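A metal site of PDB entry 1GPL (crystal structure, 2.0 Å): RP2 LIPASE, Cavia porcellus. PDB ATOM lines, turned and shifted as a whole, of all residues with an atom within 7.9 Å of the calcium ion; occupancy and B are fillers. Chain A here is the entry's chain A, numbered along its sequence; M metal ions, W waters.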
ATOM      1  N   HIS A 158      20.412   3.554  -7.930  1.00  0.00           N
ATOM      2  CA  HIS A 158      19.486   3.049  -8.942  1.00  0.00           C
ATOM      3  C   HIS A 158      20.225   2.738 -10.245  1.00  0.00           C
ATOM      4  O   HIS A 158      19.855   1.796 -10.958  1.00  0.00           O
ATOM      5  CB  HIS A 158      18.392   4.074  -9.136  1.00  0.00           C
ATOM      6  CG  HIS A 158      17.650   4.347  -7.880  1.00  0.00           C
ATOM      7  ND1 HIS A 158      16.941   3.380  -7.220  1.00  0.00           N
ATOM      8  CD2 HIS A 158      17.472   5.498  -7.175  1.00  0.00           C
ATOM      9  CE1 HIS A 158      16.342   3.916  -6.171  1.00  0.00           C
ATOM     10  NE2 HIS A 158      16.642   5.193  -6.132  1.00  0.00           N
ATOM     11  N   ALA A 160      23.192   1.434 -10.315  1.00  0.00           N
ATOM     12  CA  ALA A 160      23.743   0.105  -9.983  1.00  0.00           C
ATOM     13  C   ALA A 160      22.632  -0.927 -10.188  1.00  0.00           C
ATOM     14  O   ALA A 160      22.867  -1.992 -10.708  1.00  0.00           O
ATOM     15  CB  ALA A 160      24.240   0.064  -8.543  1.00  0.00           C
ATOM     16  N   GLY A 161      21.431  -0.545  -9.789  1.00  0.00           N
ATOM     17  CA  GLY A 161      20.243  -1.358  -9.954  1.00  0.00           C
ATOM     18  C   GLY A 161      19.936  -1.644 -11.426  1.00  0.00           C
ATOM     19  O   GLY A 161      19.611  -2.770 -11.770  1.00  0.00           O
ATOM     20  N   GLU A 162      20.010  -0.619 -12.281  1.00  0.00           N
ATOM     21  CA  GLU A 162      19.762  -0.811 -13.712  1.00  0.00           C
ATOM     22  C   GLU A 162      20.773  -1.797 -14.241  1.00  0.00           C
ATOM     23  O   GLU A 162      20.425  -2.725 -14.969  1.00  0.00           O
ATOM     24  CB  GLU A 162      19.918   0.490 -14.518  1.00  0.00           C
ATOM     25  CG  GLU A 162      18.654   1.278 -14.806  1.00  0.00           C
ATOM     26  CD  GLU A 162      17.628   0.567 -15.697  1.00  0.00           C
ATOM     27  OE1 GLU A 162      17.982  -0.151 -16.667  1.00  0.00           O
ATOM     28  OE2 GLU A 162      16.436   0.743 -15.401  1.00  0.00           O
ATOM     29  N   ALA A 163      22.033  -1.574 -13.884  1.00  0.00           N
ATOM     30  CA  ALA A 163      23.114  -2.450 -14.321  1.00  0.00           C
ATOM     31  C   ALA A 163      22.929  -3.869 -13.826  1.00  0.00           C
ATOM     32  O   ALA A 163      23.189  -4.824 -14.556  1.00  0.00           O
ATOM     33  CB  ALA A 163      24.454  -1.888 -13.907  1.00  0.00           C
ATOM     34  N   GLY A 164      22.447  -4.019 -12.601  1.00  0.00           N
ATOM     35  CA  GLY A 164      22.207  -5.352 -12.048  1.00  0.00           C
ATOM     36  C   GLY A 164      21.068  -6.049 -12.783  1.00  0.00           C
ATOM     37  O   GLY A 164      21.156  -7.242 -13.054  1.00  0.00           O
ATOM     38  N   LYS A 165      19.973  -5.337 -13.010  1.00  0.00           N
ATOM     39  CA  LYS A 165      18.816  -5.860 -13.757  1.00  0.00           C
ATOM     40  C   LYS A 165      19.217  -6.312 -15.192  1.00  0.00           C
ATOM     41  O   LYS A 165      18.818  -7.387 -15.656  1.00  0.00           O
ATOM     42  CB  LYS A 165      17.723  -4.799 -13.874  1.00  0.00           C
ATOM     43  CG  LYS A 165      16.532  -5.222 -14.724  1.00  0.00           C
ATOM     44  CD  LYS A 165      15.583  -4.078 -15.022  1.00  0.00           C
ATOM     45  CE  LYS A 165      16.233  -3.037 -15.916  1.00  0.00           C
ATOM     46  NZ  LYS A 165      15.381  -1.834 -16.126  1.00  0.00           N
ATOM     47  N   ARG A 166      20.010  -5.485 -15.871  1.00  0.00           N
ATOM     48  CA  ARG A 166      20.487  -5.755 -17.227  1.00  0.00           C
ATOM     49  C   ARG A 166      21.493  -6.885 -17.264  1.00  0.00           C
ATOM     50  O   ARG A 166      21.860  -7.369 -18.341  1.00  0.00           O
ATOM     51  CB  ARG A 166      21.055  -4.475 -17.859  1.00  0.00           C
ATOM     52  CG  ARG A 166      19.986  -3.491 -18.191  1.00  0.00           C
ATOM     53  CD  ARG A 166      20.504  -2.131 -18.518  1.00  0.00           C
ATOM     54  NE  ARG A 166      19.352  -1.279 -18.857  1.00  0.00           N
ATOM     55  CZ  ARG A 166      18.868  -1.097 -20.094  1.00  0.00           C
ATOM     56  NH1 ARG A 166      19.515  -1.616 -21.142  1.00  0.00           N
ATOM     57  NH2 ARG A 166      17.807  -0.323 -20.300  1.00  0.00           N
ATOM     58  N   ILE A 174      25.358  -5.204  -4.687  1.00  0.00           N
ATOM     59  CA  ILE A 174      25.084  -3.807  -4.954  1.00  0.00           C
ATOM     60  C   ILE A 174      24.909  -3.148  -3.579  1.00  0.00           C
ATOM     61  O   ILE A 174      24.179  -3.637  -2.754  1.00  0.00           O
ATOM     62  CB  ILE A 174      23.791  -3.571  -5.801  1.00  0.00           C
ATOM     63  CG1 ILE A 174      24.017  -3.979  -7.247  1.00  0.00           C
ATOM     64  CG2 ILE A 174      23.338  -2.090  -5.688  1.00  0.00           C
ATOM     65  CD1 ILE A 174      22.836  -3.787  -8.108  1.00  0.00           C
ATOM     66  N   PRO A 188       7.974   0.384  -9.901  1.00  0.00           N
ATOM     67  CA  PRO A 188       8.173  -1.061 -10.027  1.00  0.00           C
ATOM     68  C   PRO A 188       9.653  -1.433  -9.923  1.00  0.00           C
ATOM     69  O   PRO A 188      10.509  -0.575 -10.052  1.00  0.00           O
ATOM     70  CB  PRO A 188       7.606  -1.358 -11.413  1.00  0.00           C
ATOM     71  CG  PRO A 188       6.496  -0.365 -11.525  1.00  0.00           C
ATOM     72  CD  PRO A 188       7.180   0.895 -11.044  1.00  0.00           C
ATOM     73  N   GLU A 189       9.939  -2.708  -9.663  1.00  0.00           N
ATOM     74  CA  GLU A 189      11.312  -3.186  -9.526  1.00  0.00           C
ATOM     75  C   GLU A 189      12.274  -2.842 -10.669  1.00  0.00           C
ATOM     76  O   GLU A 189      13.502  -2.767 -10.460  1.00  0.00           O
ATOM     77  CB  GLU A 189      11.342  -4.705  -9.307  1.00  0.00           C
ATOM     78  CG  GLU A 189      10.873  -5.159  -7.961  1.00  0.00           C
ATOM     79  CD  GLU A 189       9.508  -5.788  -8.024  1.00  0.00           C
ATOM     80  OE1 GLU A 189       8.507  -5.040  -7.927  1.00  0.00           O
ATOM     81  OE2 GLU A 189       9.444  -7.026  -8.180  1.00  0.00           O
ATOM     82  N   GLU A 190      11.746  -2.783 -11.901  1.00  0.00           N
ATOM     83  CA  GLU A 190      12.546  -2.490 -13.104  1.00  0.00           C
ATOM     84  C   GLU A 190      13.102  -1.067 -13.110  1.00  0.00           C
ATOM     85  O   GLU A 190      14.140  -0.822 -13.714  1.00  0.00           O
ATOM     86  CB  GLU A 190      11.739  -2.679 -14.383  1.00  0.00           C
ATOM     87  CG  GLU A 190      10.731  -3.797 -14.377  1.00  0.00           C
ATOM     88  CD  GLU A 190       9.398  -3.387 -13.794  1.00  0.00           C
ATOM     89  OE1 GLU A 190       8.711  -2.524 -14.395  1.00  0.00           O
ATOM     90  OE2 GLU A 190       9.046  -3.933 -12.730  1.00  0.00           O
ATOM     91  N   VAL A 191      12.412  -0.145 -12.453  1.00  0.00           N
ATOM     92  CA  VAL A 191      12.830   1.241 -12.377  1.00  0.00           C
ATOM     93  C   VAL A 191      13.861   1.519 -11.267  1.00  0.00           C
ATOM     94  O   VAL A 191      14.861   2.193 -11.500  1.00  0.00           O
ATOM     95  CB  VAL A 191      11.603   2.165 -12.156  1.00  0.00           C
ATOM     96  CG1 VAL A 191      12.029   3.598 -12.023  1.00  0.00           C
ATOM     97  CG2 VAL A 191      10.597   2.007 -13.297  1.00  0.00           C
ATOM     98  N   ARG A 192      13.646   0.915 -10.089  1.00  0.00           N
ATOM     99  CA  ARG A 192      14.485   1.109  -8.890  1.00  0.00           C
ATOM    100  C   ARG A 192      15.345  -0.071  -8.419  1.00  0.00           C
ATOM    101  O   ARG A 192      15.189  -1.243  -8.844  1.00  0.00           O
ATOM    102  CB  ARG A 192      13.592   1.548  -7.718  1.00  0.00           C
ATOM    103  CG  ARG A 192      12.680   0.426  -7.268  1.00  0.00           C
ATOM    104  CD  ARG A 192      11.801   0.809  -6.107  1.00  0.00           C
ATOM    105  NE  ARG A 192      10.871  -0.270  -5.761  1.00  0.00           N
ATOM    106  CZ  ARG A 192      11.194  -1.421  -5.160  1.00  0.00           C
ATOM    107  NH1 ARG A 192      12.443  -1.686  -4.805  1.00  0.00           N
ATOM    108  NH2 ARG A 192      10.255  -2.333  -4.934  1.00  0.00           N
ATOM    109  N   LEU A 193      16.286   0.258  -7.519  1.00  0.00           N
ATOM    110  CA  LEU A 193      17.164  -0.737  -6.912  1.00  0.00           C
ATOM    111  C   LEU A 193      16.213  -1.600  -6.072  1.00  0.00           C
ATOM    112  O   LEU A 193      15.243  -1.110  -5.508  1.00  0.00           O
ATOM    113  CB  LEU A 193      18.207  -0.052  -6.009  1.00  0.00           C
ATOM    114  CG  LEU A 193      19.152  -0.924  -5.183  1.00  0.00           C
ATOM    115  CD1 LEU A 193      19.899  -1.838  -6.093  1.00  0.00           C
ATOM    116  CD2 LEU A 193      20.144  -0.059  -4.409  1.00  0.00           C
ATOM    117  N   ASP A 194      16.414  -2.905  -6.107  1.00  0.00           N
ATOM    118  CA  ASP A 194      15.583  -3.810  -5.334  1.00  0.00           C
ATOM    119  C   ASP A 194      16.460  -5.042  -5.124  1.00  0.00           C
ATOM    120  O   ASP A 194      17.455  -5.207  -5.806  1.00  0.00           O
ATOM    121  CB  ASP A 194      14.236  -4.090  -6.042  1.00  0.00           C
ATOM    122  CG  ASP A 194      14.368  -5.008  -7.244  1.00  0.00           C
ATOM    123  OD1 ASP A 194      14.661  -4.516  -8.343  1.00  0.00           O
ATOM    124  OD2 ASP A 194      14.143  -6.216  -7.094  1.00  0.00           O
ATOM    125  N   PRO A 195      16.093  -5.920  -4.195  1.00  0.00           N
ATOM    126  CA  PRO A 195      16.855  -7.122  -3.890  1.00  0.00           C
ATOM    127  C   PRO A 195      17.241  -8.004  -5.068  1.00  0.00           C
ATOM    128  O   PRO A 195      18.312  -8.623  -5.051  1.00  0.00           O
ATOM    129  CB  PRO A 195      15.941  -7.868  -2.929  1.00  0.00           C
ATOM    130  CG  PRO A 195      15.272  -6.757  -2.199  1.00  0.00           C
ATOM    131  CD  PRO A 195      14.891  -5.859  -3.341  1.00  0.00           C
ATOM    132  N   SER A 196      16.381  -8.035  -6.093  1.00  0.00           N
ATOM    133  CA  SER A 196      16.601  -8.887  -7.277  1.00  0.00           C
ATOM    134  C   SER A 196      17.711  -8.445  -8.194  1.00  0.00           C
ATOM    135  O   SER A 196      18.160  -9.244  -8.981  1.00  0.00           O
ATOM    136  CB  SER A 196      15.330  -9.047  -8.101  1.00  0.00           C
ATOM    137  OG  SER A 196      15.036  -7.847  -8.796  1.00  0.00           O
ATOM    138  N   ASP A 197      18.174  -7.202  -8.045  1.00  0.00           N
ATOM    139  CA  ASP A 197      19.220  -6.671  -8.903  1.00  0.00           C
ATOM    140  C   ASP A 197      20.603  -7.227  -8.727  1.00  0.00           C
ATOM    141  O   ASP A 197      21.463  -6.986  -9.568  1.00  0.00           O
ATOM    142  CB  ASP A 197      19.279  -5.145  -8.820  1.00  0.00           C
ATOM    143  CG  ASP A 197      17.997  -4.490  -9.226  1.00  0.00           C
ATOM    144  OD1 ASP A 197      17.246  -5.059 -10.052  1.00  0.00           O
ATOM    145  OD2 ASP A 197      17.720  -3.400  -8.724  1.00  0.00           O
ATOM    146  N   ALA A 198      20.845  -7.904  -7.613  1.00  0.00           N
ATOM    147  CA  ALA A 198      22.173  -8.480  -7.353  1.00  0.00           C
ATOM    148  C   ALA A 198      22.001  -9.640  -6.367  1.00  0.00           C
ATOM    149  O   ALA A 198      20.938  -9.784  -5.763  1.00  0.00           O
ATOM    150  CB  ALA A 198      23.097  -7.414  -6.783  1.00  0.00           C
ATOM    151  N   VAL A 223      14.956  -1.310   0.304  1.00  0.00           N
ATOM    152  CA  VAL A 223      15.287  -1.745  -1.058  1.00  0.00           C
ATOM    153  C   VAL A 223      16.345  -2.853  -1.200  1.00  0.00           C
ATOM    154  O   VAL A 223      16.654  -3.264  -2.324  1.00  0.00           O
ATOM    155  CB  VAL A 223      15.687  -0.523  -1.948  1.00  0.00           C
ATOM    156  CG1 VAL A 223      14.598   0.520  -1.964  1.00  0.00           C
ATOM    157  CG2 VAL A 223      16.974   0.105  -1.490  1.00  0.00           C
HETATM  158 CA    CA M   1      15.425  -3.336 -10.017  1.00  0.00          CA
HETATM  159  O   HOH W   1      14.771  -5.069 -11.445  1.00  0.00           O
HETATM  160  O   HOH W   2      16.473  -2.105 -11.694  1.00  0.00           O
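The calcium ion is bound by O of Glu 189, OD1 of Asp 194, water W2, water W1, O of Arg 192, OD1 of Asp 197 and OD2 of Asp 197.
Within 4 Å of the calcium ion: Glu 189, Arg 192, Asp 194 and Asp 197.
The side-chain hydroxyl (OG) of Ser 196 sits at hydrogen-bond distance from the side-chain carboxylate (OD2) of Asp 194.
Water W2 bridges O of Gly 161 (3.2 Å) and O of Glu 190 (3.3 Å).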
